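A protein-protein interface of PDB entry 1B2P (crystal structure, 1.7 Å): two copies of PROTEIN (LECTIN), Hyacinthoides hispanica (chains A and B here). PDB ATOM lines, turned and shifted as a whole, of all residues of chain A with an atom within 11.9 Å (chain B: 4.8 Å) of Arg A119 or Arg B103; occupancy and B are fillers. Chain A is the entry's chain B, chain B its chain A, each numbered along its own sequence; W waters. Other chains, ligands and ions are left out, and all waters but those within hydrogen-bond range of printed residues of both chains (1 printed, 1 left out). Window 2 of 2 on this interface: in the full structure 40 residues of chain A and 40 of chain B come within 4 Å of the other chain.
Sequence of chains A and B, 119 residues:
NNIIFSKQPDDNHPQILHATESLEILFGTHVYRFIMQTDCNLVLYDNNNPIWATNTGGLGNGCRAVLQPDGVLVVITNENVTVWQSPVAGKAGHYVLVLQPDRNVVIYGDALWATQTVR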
ATOM      1  N   ILE A   3      -3.594   5.934  14.497  1.00  0.00           N
ATOM      2  CA  ILE A   3      -2.268   6.399  14.940  1.00  0.00           C
ATOM      3  C   ILE A   3      -2.435   7.725  15.714  1.00  0.00           C
ATOM      4  O   ILE A   3      -3.396   8.502  15.467  1.00  0.00           O
ATOM      5  CB  ILE A   3      -1.443   6.684  13.637  1.00  0.00           C
ATOM      6  CG1 ILE A   3      -0.090   7.233  13.976  1.00  0.00           C
ATOM      7  CG2 ILE A   3      -2.164   7.694  12.725  1.00  0.00           C
ATOM      8  CD1 ILE A   3       0.819   6.747  12.747  1.00  0.00           C
ATOM      9  N   PHE A   5       0.134  10.904  16.747  1.00  0.00           N
ATOM     10  CA  PHE A   5       1.488  11.400  16.584  1.00  0.00           C
ATOM     11  C   PHE A   5       1.951  12.201  17.804  1.00  0.00           C
ATOM     12  O   PHE A   5       1.118  12.774  18.533  1.00  0.00           O
ATOM     13  CB  PHE A   5       1.357  12.492  15.429  1.00  0.00           C
ATOM     14  CG  PHE A   5       1.059  11.796  14.094  1.00  0.00           C
ATOM     15  CD1 PHE A   5       2.138  11.379  13.318  1.00  0.00           C
ATOM     16  CD2 PHE A   5      -0.227  11.750  13.631  1.00  0.00           C
ATOM     17  CE1 PHE A   5       1.884  10.771  12.078  1.00  0.00           C
ATOM     18  CE2 PHE A   5      -0.535  11.127  12.396  1.00  0.00           C
ATOM     19  CZ  PHE A   5       0.564  10.686  11.668  1.00  0.00           C
ATOM     20  N   GLN A   8       3.973  17.952  18.307  1.00  0.00           N
ATOM     21  CA  GLN A   8       4.934  18.571  17.338  1.00  0.00           C
ATOM     22  C   GLN A   8       4.140  19.654  16.571  1.00  0.00           C
ATOM     23  O   GLN A   8       2.935  19.691  16.420  1.00  0.00           O
ATOM     24  CB  GLN A   8       5.343  17.511  16.329  1.00  0.00           C
ATOM     25  CG  GLN A   8       4.185  16.837  15.534  1.00  0.00           C
ATOM     26  CD  GLN A   8       4.793  15.617  14.767  1.00  0.00           C
ATOM     27  OE1 GLN A   8       5.284  15.684  13.629  1.00  0.00           O
ATOM     28  NE2 GLN A   8       4.780  14.463  15.432  1.00  0.00           N
ATOM     29  N   PRO A   9       4.936  20.672  16.147  1.00  0.00           N
ATOM     30  CA  PRO A   9       4.252  21.823  15.567  1.00  0.00           C
ATOM     31  C   PRO A   9       3.997  21.687  14.106  1.00  0.00           C
ATOM     32  O   PRO A   9       4.585  22.366  13.266  1.00  0.00           O
ATOM     33  CB  PRO A   9       5.352  22.904  15.923  1.00  0.00           C
ATOM     34  CG  PRO A   9       6.661  22.223  15.749  1.00  0.00           C
ATOM     35  CD  PRO A   9       6.378  20.797  16.417  1.00  0.00           C
ATOM     36  N   ASP A  10       3.152  20.797  13.601  1.00  0.00           N
ATOM     37  CA  ASP A  10       2.880  20.508  12.214  1.00  0.00           C
ATOM     38  C   ASP A  10       1.436  19.976  12.197  1.00  0.00           C
ATOM     39  O   ASP A  10       0.829  19.831  13.268  1.00  0.00           O
ATOM     40  CB  ASP A  10       3.937  19.694  11.560  1.00  0.00           C
ATOM     41  CG  ASP A  10       4.057  18.261  12.161  1.00  0.00           C
ATOM     42  OD1 ASP A  10       2.973  17.758  12.430  1.00  0.00           O
ATOM     43  OD2 ASP A  10       5.183  17.935  12.424  1.00  0.00           O
ATOM     44  N   ASP A  11       0.893  19.707  11.042  1.00  0.00           N
ATOM     45  CA  ASP A  11      -0.514  19.367  11.118  1.00  0.00           C
ATOM     46  C   ASP A  11      -0.637  17.795  11.038  1.00  0.00           C
ATOM     47  O   ASP A  11      -1.776  17.468  10.691  1.00  0.00           O
ATOM     48  CB  ASP A  11      -1.487  20.051  10.168  1.00  0.00           C
ATOM     49  CG  ASP A  11      -0.770  20.216   8.863  1.00  0.00           C
ATOM     50  OD1 ASP A  11      -0.127  19.222   8.428  1.00  0.00           O
ATOM     51  OD2 ASP A  11      -0.900  21.374   8.344  1.00  0.00           O
ATOM     52  N   ASN A  12       0.345  17.139  11.632  1.00  0.00           N
ATOM     53  CA  ASN A  12      -0.009  15.695  11.843  1.00  0.00           C
ATOM     54  C   ASN A  12      -1.021  15.581  12.977  1.00  0.00           C
ATOM     55  O   ASN A  12      -0.879  16.335  13.920  1.00  0.00           O
ATOM     56  CB  ASN A  12       1.256  14.974  12.187  1.00  0.00           C
ATOM     57  CG  ASN A  12       2.242  14.817  11.030  1.00  0.00           C
ATOM     58  OD1 ASN A  12       3.456  14.792  11.254  1.00  0.00           O
ATOM     59  ND2 ASN A  12       1.676  14.648   9.930  1.00  0.00           N
ATOM     60  N   HIS A  13      -2.050  14.861  12.740  1.00  0.00           N
ATOM     61  CA  HIS A  13      -3.137  14.751  13.706  1.00  0.00           C
ATOM     62  C   HIS A  13      -3.739  13.384  13.634  1.00  0.00           C
ATOM     63  O   HIS A  13      -3.600  12.794  12.563  1.00  0.00           O
ATOM     64  CB  HIS A  13      -4.264  15.798  13.381  1.00  0.00           C
ATOM     65  CG  HIS A  13      -4.802  15.508  12.006  1.00  0.00           C
ATOM     66  ND1 HIS A  13      -5.978  14.775  11.827  1.00  0.00           N
ATOM     67  CD2 HIS A  13      -4.330  15.802  10.732  1.00  0.00           C
ATOM     68  CE1 HIS A  13      -6.209  14.644  10.511  1.00  0.00           C
ATOM     69  NE2 HIS A  13      -5.240  15.251   9.856  1.00  0.00           N
ATOM     70  N   GLN A  15      -2.894  14.445  17.707  1.00  0.00           N
ATOM     71  CA  GLN A  15      -1.818  14.386  18.646  1.00  0.00           C
ATOM     72  C   GLN A  15      -2.414  14.257  20.067  1.00  0.00           C
ATOM     73  O   GLN A  15      -1.561  13.898  20.909  1.00  0.00           O
ATOM     74  CB  GLN A  15      -0.980  15.741  18.674  1.00  0.00           C
ATOM     75  CG  GLN A  15      -0.304  15.903  17.322  1.00  0.00           C
ATOM     76  CD  GLN A  15       0.595  17.167  17.215  1.00  0.00           C
ATOM     77  OE1 GLN A  15       0.961  17.666  18.261  1.00  0.00           O
ATOM     78  NE2 GLN A  15       0.744  17.494  15.967  1.00  0.00           N
ATOM     79  N   TRP A 113      14.243   7.878   9.199  1.00  0.00           N
ATOM     80  CA  TRP A 113      14.499   8.432   7.831  1.00  0.00           C
ATOM     81  C   TRP A 113      13.203   8.932   7.379  1.00  0.00           C
ATOM     82  O   TRP A 113      12.072   8.461   7.717  1.00  0.00           O
ATOM     83  CB  TRP A 113      15.044   7.286   6.930  1.00  0.00           C
ATOM     84  CG  TRP A 113      15.152   7.747   5.498  1.00  0.00           C
ATOM     85  CD1 TRP A 113      16.251   8.450   4.970  1.00  0.00           C
ATOM     86  CD2 TRP A 113      14.233   7.568   4.453  1.00  0.00           C
ATOM     87  NE1 TRP A 113      16.000   8.662   3.606  1.00  0.00           N
ATOM     88  CE2 TRP A 113      14.801   8.161   3.262  1.00  0.00           C
ATOM     89  CE3 TRP A 113      12.963   6.995   4.399  1.00  0.00           C
ATOM     90  CZ2 TRP A 113      14.082   8.121   2.099  1.00  0.00           C
ATOM     91  CZ3 TRP A 113      12.247   6.981   3.197  1.00  0.00           C
ATOM     92  CH2 TRP A 113      12.866   7.560   2.015  1.00  0.00           C
ATOM     93  N   ALA A 114      13.192   9.959   6.487  1.00  0.00           N
ATOM     94  CA  ALA A 114      12.022  10.467   5.858  1.00  0.00           C
ATOM     95  C   ALA A 114      12.232  10.989   4.441  1.00  0.00           C
ATOM     96  O   ALA A 114      13.421  11.220   4.153  1.00  0.00           O
ATOM     97  CB  ALA A 114      11.464  11.695   6.679  1.00  0.00           C
ATOM     98  N   THR A 115      11.175  11.029   3.682  1.00  0.00           N
ATOM     99  CA  THR A 115      11.316  11.628   2.302  1.00  0.00           C
ATOM    100  C   THR A 115      11.582  13.138   2.377  1.00  0.00           C
ATOM    101  O   THR A 115      12.030  13.618   1.270  1.00  0.00           O
ATOM    102  CB  THR A 115      10.067  11.319   1.517  1.00  0.00           C
ATOM    103  OG1 THR A 115       8.907  11.726   2.280  1.00  0.00           O
ATOM    104  CG2 THR A 115       9.921   9.810   1.164  1.00  0.00           C
ATOM    105  N   GLN A 116      11.181  13.766   3.424  1.00  0.00           N
ATOM    106  CA  GLN A 116      11.299  15.225   3.603  1.00  0.00           C
ATOM    107  C   GLN A 116      10.451  15.928   2.596  1.00  0.00           C
ATOM    108  O   GLN A 116      10.928  16.853   1.878  1.00  0.00           O
ATOM    109  CB  GLN A 116      12.765  15.613   3.492  1.00  0.00           C
ATOM    110  CG  GLN A 116      13.658  14.943   4.527  1.00  0.00           C
ATOM    111  CD  GLN A 116      15.140  15.245   4.443  1.00  0.00           C
ATOM    112  OE1 GLN A 116      15.718  15.517   5.501  1.00  0.00           O
ATOM    113  NE2 GLN A 116      15.780  15.194   3.283  1.00  0.00           N
ATOM    114  N   THR A 117       9.174  15.637   2.513  1.00  0.00           N
ATOM    115  CA  THR A 117       8.243  16.135   1.501  1.00  0.00           C
ATOM    116  C   THR A 117       7.108  16.901   2.183  1.00  0.00           C
ATOM    117  O   THR A 117       6.027  16.944   1.596  1.00  0.00           O
ATOM    118  CB  THR A 117       7.672  15.005   0.655  1.00  0.00           C
ATOM    119  OG1 THR A 117       7.328  13.912   1.574  1.00  0.00           O
ATOM    120  CG2 THR A 117       8.734  14.444  -0.296  1.00  0.00           C
ATOM    121  N   VAL A 118       7.393  17.445   3.350  1.00  0.00           N
ATOM    122  CA  VAL A 118       6.367  18.216   4.075  1.00  0.00           C
ATOM    123  C   VAL A 118       5.775  19.332   3.213  1.00  0.00           C
ATOM    124  O   VAL A 118       6.544  20.015   2.559  1.00  0.00           O
ATOM    125  CB  VAL A 118       6.931  18.799   5.385  1.00  0.00           C
ATOM    126  CG1 VAL A 118       5.865  19.667   6.065  1.00  0.00           C
ATOM    127  CG2 VAL A 118       7.273  17.649   6.359  1.00  0.00           C
ATOM    128  N   ARG A 119       4.472  19.409   3.073  1.00  0.00           N
ATOM    129  CA  ARG A 119       3.773  20.632   2.759  1.00  0.00           C
ATOM    130  C   ARG A 119       2.435  20.391   2.101  1.00  0.00           C
ATOM    131  O   ARG A 119       1.584  19.745   2.738  1.00  0.00           O
ATOM    132  CB  ARG A 119       4.610  21.660   1.986  1.00  0.00           C
ATOM    133  CG  ARG A 119       4.879  22.863   2.876  1.00  0.00           C
ATOM    134  CD  ARG A 119       6.207  22.700   3.613  1.00  0.00           C
ATOM    135  NE  ARG A 119       7.211  23.558   2.980  1.00  0.00           N
ATOM    136  CZ  ARG A 119       8.172  24.232   3.607  1.00  0.00           C
ATOM    137  NH1 ARG A 119       8.285  24.115   4.936  1.00  0.00           N
ATOM    138  NH2 ARG A 119       9.021  24.999   2.918  1.00  0.00           N
ATOM    139  OXT ARG A 119       2.128  20.898   0.991  1.00  0.00           O
ATOM    140  N   TYR B  32      -2.975  11.906  -1.236  1.00  0.00           N
ATOM    141  CA  TYR B  32      -1.490  11.668  -1.196  1.00  0.00           C
ATOM    142  C   TYR B  32      -1.389  10.178  -1.439  1.00  0.00           C
ATOM    143  O   TYR B  32      -2.132   9.434  -0.827  1.00  0.00           O
ATOM    144  CB  TYR B  32      -0.920  12.007   0.135  1.00  0.00           C
ATOM    145  CG  TYR B  32      -0.953  13.477   0.481  1.00  0.00           C
ATOM    146  CD1 TYR B  32      -0.988  14.458  -0.514  1.00  0.00           C
ATOM    147  CD2 TYR B  32      -0.878  13.820   1.810  1.00  0.00           C
ATOM    148  CE1 TYR B  32      -1.035  15.781  -0.081  1.00  0.00           C
ATOM    149  CE2 TYR B  32      -0.856  15.176   2.231  1.00  0.00           C
ATOM    150  CZ  TYR B  32      -0.955  16.101   1.230  1.00  0.00           C
ATOM    151  OH  TYR B  32      -0.908  17.453   1.604  1.00  0.00           O
ATOM    152  N   LEU B  44       5.810   9.150  -4.606  1.00  0.00           N
ATOM    153  CA  LEU B  44       4.781   9.860  -3.777  1.00  0.00           C
ATOM    154  C   LEU B  44       4.137  10.954  -4.673  1.00  0.00           C
ATOM    155  O   LEU B  44       4.854  11.778  -5.218  1.00  0.00           O
ATOM    156  CB  LEU B  44       5.480  10.532  -2.635  1.00  0.00           C
ATOM    157  CG  LEU B  44       4.615  11.429  -1.698  1.00  0.00           C
ATOM    158  CD1 LEU B  44       3.617  10.518  -0.958  1.00  0.00           C
ATOM    159  CD2 LEU B  44       5.577  12.095  -0.740  1.00  0.00           C
ATOM    160  N   ASP B  46       1.151  13.967  -5.037  1.00  0.00           N
ATOM    161  CA  ASP B  46       0.121  14.846  -4.387  1.00  0.00           C
ATOM    162  C   ASP B  46      -0.890  15.039  -5.462  1.00  0.00           C
ATOM    163  O   ASP B  46      -0.519  15.686  -6.488  1.00  0.00           O
ATOM    164  CB  ASP B  46       0.816  16.133  -3.927  1.00  0.00           C
ATOM    165  CG  ASP B  46      -0.149  17.184  -3.311  1.00  0.00           C
ATOM    166  OD1 ASP B  46      -1.327  17.044  -3.569  1.00  0.00           O
ATOM    167  OD2 ASP B  46       0.454  18.000  -2.606  1.00  0.00           O
ATOM    168  N   ILE B  51       5.906  14.110  -6.362  1.00  0.00           N
ATOM    169  CA  ILE B  51       6.707  14.957  -5.513  1.00  0.00           C
ATOM    170  C   ILE B  51       7.988  14.346  -4.985  1.00  0.00           C
ATOM    171  O   ILE B  51       8.886  15.037  -4.503  1.00  0.00           O
ATOM    172  CB  ILE B  51       5.983  15.684  -4.390  1.00  0.00           C
ATOM    173  CG1 ILE B  51       5.427  14.654  -3.446  1.00  0.00           C
ATOM    174  CG2 ILE B  51       4.825  16.544  -5.035  1.00  0.00           C
ATOM    175  CD1 ILE B  51       4.795  15.293  -2.186  1.00  0.00           C
ATOM    176  N   GLN B 100       2.056  10.416   6.182  1.00  0.00           N
ATOM    177  CA  GLN B 100       1.454  11.306   7.263  1.00  0.00           C
ATOM    178  C   GLN B 100       0.655  12.418   6.700  1.00  0.00           C
ATOM    179  O   GLN B 100       0.825  12.828   5.527  1.00  0.00           O
ATOM    180  CB  GLN B 100       2.630  12.007   7.956  1.00  0.00           C
ATOM    181  CG  GLN B 100       3.556  10.911   8.590  1.00  0.00           C
ATOM    182  CD  GLN B 100       4.581  11.446   9.499  1.00  0.00           C
ATOM    183  OE1 GLN B 100       5.120  10.706  10.347  1.00  0.00           O
ATOM    184  NE2 GLN B 100       5.083  12.707   9.403  1.00  0.00           N
ATOM    185  N   PRO B 101      -0.275  12.999   7.504  1.00  0.00           N
ATOM    186  CA  PRO B 101      -1.119  14.065   6.976  1.00  0.00           C
ATOM    187  C   PRO B 101      -0.252  15.252   6.590  1.00  0.00           C
ATOM    188  O   PRO B 101      -0.812  16.006   5.745  1.00  0.00           O
ATOM    189  CB  PRO B 101      -1.893  14.482   8.270  1.00  0.00           C
ATOM    190  CG  PRO B 101      -2.060  13.115   8.983  1.00  0.00           C
ATOM    191  CD  PRO B 101      -0.712  12.442   8.831  1.00  0.00           C
ATOM    192  N   ASP B 102       0.922  15.443   7.095  1.00  0.00           N
ATOM    193  CA  ASP B 102       1.700  16.614   6.667  1.00  0.00           C
ATOM    194  C   ASP B 102       2.444  16.331   5.345  1.00  0.00           C
ATOM    195  O   ASP B 102       3.215  17.186   4.956  1.00  0.00           O
ATOM    196  CB  ASP B 102       2.656  17.080   7.761  1.00  0.00           C
ATOM    197  CG  ASP B 102       3.812  16.268   8.117  1.00  0.00           C
ATOM    198  OD1 ASP B 102       3.911  15.143   7.510  1.00  0.00           O
ATOM    199  OD2 ASP B 102       4.676  16.548   8.965  1.00  0.00           O
ATOM    200  N   ARG B 103       2.198  15.215   4.725  1.00  0.00           N
ATOM    201  CA  ARG B 103       2.735  14.837   3.377  1.00  0.00           C
ATOM    202  C   ARG B 103       4.147  14.332   3.524  1.00  0.00           C
ATOM    203  O   ARG B 103       4.682  13.927   2.504  1.00  0.00           O
ATOM    204  CB  ARG B 103       2.676  16.020   2.348  1.00  0.00           C
ATOM    205  CG  ARG B 103       2.490  15.421   0.901  1.00  0.00           C
ATOM    206  CD  ARG B 103       2.499  16.694  -0.085  1.00  0.00           C
ATOM    207  NE  ARG B 103       3.801  17.339  -0.026  1.00  0.00           N
ATOM    208  CZ  ARG B 103       4.014  18.366  -0.988  1.00  0.00           C
ATOM    209  NH1 ARG B 103       3.081  18.627  -1.862  1.00  0.00           N
ATOM    210  NH2 ARG B 103       5.199  18.911  -0.866  1.00  0.00           N
ATOM    211  N   ASN B 104       4.723  14.111   4.718  1.00  0.00           N
ATOM    212  CA  ASN B 104       6.007  13.446   4.809  1.00  0.00           C
ATOM    213  C   ASN B 104       5.807  11.901   4.911  1.00  0.00           C
ATOM    214  O   ASN B 104       4.690  11.554   5.332  1.00  0.00           O
ATOM    215  CB  ASN B 104       6.654  13.932   6.097  1.00  0.00           C
ATOM    216  CG  ASN B 104       8.165  13.974   6.048  1.00  0.00           C
ATOM    217  OD1 ASN B 104       8.758  13.689   5.009  1.00  0.00           O
ATOM    218  ND2 ASN B 104       8.792  14.308   7.180  1.00  0.00           N
ATOM    219  N   VAL B 105       6.766  11.226   4.376  1.00  0.00           N
ATOM    220  CA  VAL B 105       6.655   9.683   4.609  1.00  0.00           C
ATOM    221  C   VAL B 105       7.844   9.370   5.442  1.00  0.00           C
ATOM    222  O   VAL B 105       9.000   9.744   5.189  1.00  0.00           O
ATOM    223  CB  VAL B 105       6.912   8.990   3.254  1.00  0.00           C
ATOM    224  CG1 VAL B 105       7.113   7.476   3.499  1.00  0.00           C
ATOM    225  CG2 VAL B 105       5.719   9.245   2.348  1.00  0.00           C
HETATM  226  O   HOH W   1       6.597  14.250  11.769  1.00  0.00           O
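O of Val B105 lies within hydrogen-bond range of N of Thr A115, at 2.9 Å.
The side-chain amide nitrogen (NE2) of Gln B100 lies within hydrogen-bond range of the side-chain amide oxygen (OD1) of Asn A12.
The side-chain amide nitrogen of Asn A12 lies close to the backbone NH of Asp B102, at 3.0 Å.
NE of Arg B103 sits at hydrogen-bond distance from O of Thr A117.
The side-chain hydroxyl of Thr A115 is in hydrogen-bond range of the side-chain amide oxygen of Asn B104 (3.4 Å).
The backbone carbonyl oxygen (O) of Asp B102 lies within hydrogen-bond range of the backbone NH (N) of Arg A119, 3.2 Å away.
The chain-end carboxylate of Arg A119 lies within salt-bridge range of the guanidinium group of Arg B103, at 3.8 Å.
OD1 of Asn B104 lies within hydrogen-bond range of N of Gln A116, 2.9 Å away.
The side-chain amide oxygen of Asn B104 lies within hydrogen-bond range of the backbone NH of Thr A117.
NH1 of Arg B103 is in salt-bridge range of OD2 of Asp B46 (2.8 Å).
The side-chain amide oxygen of Gln A8 sits close to the side-chain carboxylate of Asp A10 (2.6 Å).
The backbone NH of Asn B104 is in hydrogen-bond range of the side-chain carboxylate of Asp B102 (3.1 Å).
The backbone carbonyl oxygen (O) of Leu B44 is in hydrogen-bond range of the backbone NH (N) of Ile B51, 2.8 Å away.
The side-chain hydroxyl of Thr A117 sits at hydrogen-bond distance from the side-chain hydroxyl of Thr A115, at 2.8 Å.
The side-chain carboxylate (OD1) of Asp A10 is in hydrogen-bond range of the backbone NH (N) of Asn A12 (2.8 Å).
Among the printed residues, merely in contact across the chains: Phe A5 with Gln B100 (3.7 Å), Phe A5 with Pro B101 (3.6 Å), Asp A10 with Asp B102 (3.7 Å), Asp A11 with Pro B101 (3.8 Å), Asp A11 with Asp B102 (3.6 Å), Asn A12 with Pro B101 (3.4 Å), His A13 with Pro B101 (3.7 Å), Ala A114 with Asn B104 (3.8 Å), Ala A114 with Val B105 (3.2 Å), Thr A117 with Leu B44 (3.4 Å), Thr A117 with Val B105 (3.9 Å), Val A118 with Asp B102 (3.4 Å), Val A118 with Arg B103 (3.8 Å), Val A118 with Asn B104 (3.8 Å) and Arg A119 with Tyr B32 (3.6 Å).
Ile A3 touches none of the printed residues of chain B.
Printed residues of chain B within 4 Å of Phe A5: Gln B100 and Pro B101.
Printed residues of chain B within 4 Å of Asp A10: Asp B102.
Of the printed residues of chain B, His A13 touches Pro B101 (3.7 Å).
Of the printed residues of chain B, Thr A115 touches Asn B104 (3.4 Å) and Val B105 (2.9 Å).
Arg A119 touches just these residues of chain B: Tyr B32, Asp B102 and Arg B103.
Of chain A, only Arg A119 (3.6 Å) comes within 4 Å of Tyr B32.
Gln B100 touches two residues of chain A.
Of chain A, only Asp A10, Asp A11, Asn A12, Val A118 and Arg A119 come within 4 Å of Asp B102.
Asn B104 touches just these residues of chain A: Ala A114 (3.8 Å), Thr A115 (3.4 Å), Gln A116 (2.9 Å), Thr A117 (3.2 Å) and Val A118 (3.8 Å).
Val B105 touches just these residues of chain A: Ala A114 (3.2 Å), Thr A115 (2.9 Å) and Thr A117 (3.9 Å).
The nearest printed residue of chain B that does not touch Arg A119 is Asp B46 (4.9 Å).
The nearest residue of chain A that does not touch Arg B103 is Thr A115 (4.8 Å).
Hydrophobic or aromatic side chains of chain A that line the printed part of chain B: Phe A5, His A13, Ala A114 and Val A118.
Of the 10 printed residues of chain B, 8 touch a printed residue of chain A.
Hydrophobic or aromatic side chains of chain B within 4 Å of the printed part of chain A: Tyr B32, Leu B44, Pro B101 and Val B105.
Among the printed residues, 24 pairs touch across the chains.
Among the printed residues, no Asp or Glu carboxylate lies within 4 Å of a Lys or Arg side-chain nitrogen of the other chain.
No position is printed for both chains.
Of the 24 pairs that touch across the chains among the printed residues, none has its exchanged pair printed and touching as well.
Water W1 lies within hydrogen-bond range of the side-chain amide oxygen (OE1) of Gln A8, the side-chain amide nitrogen (NE2) of Gln B100 and the side-chain amide oxygen (OD1) of Asn A12.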
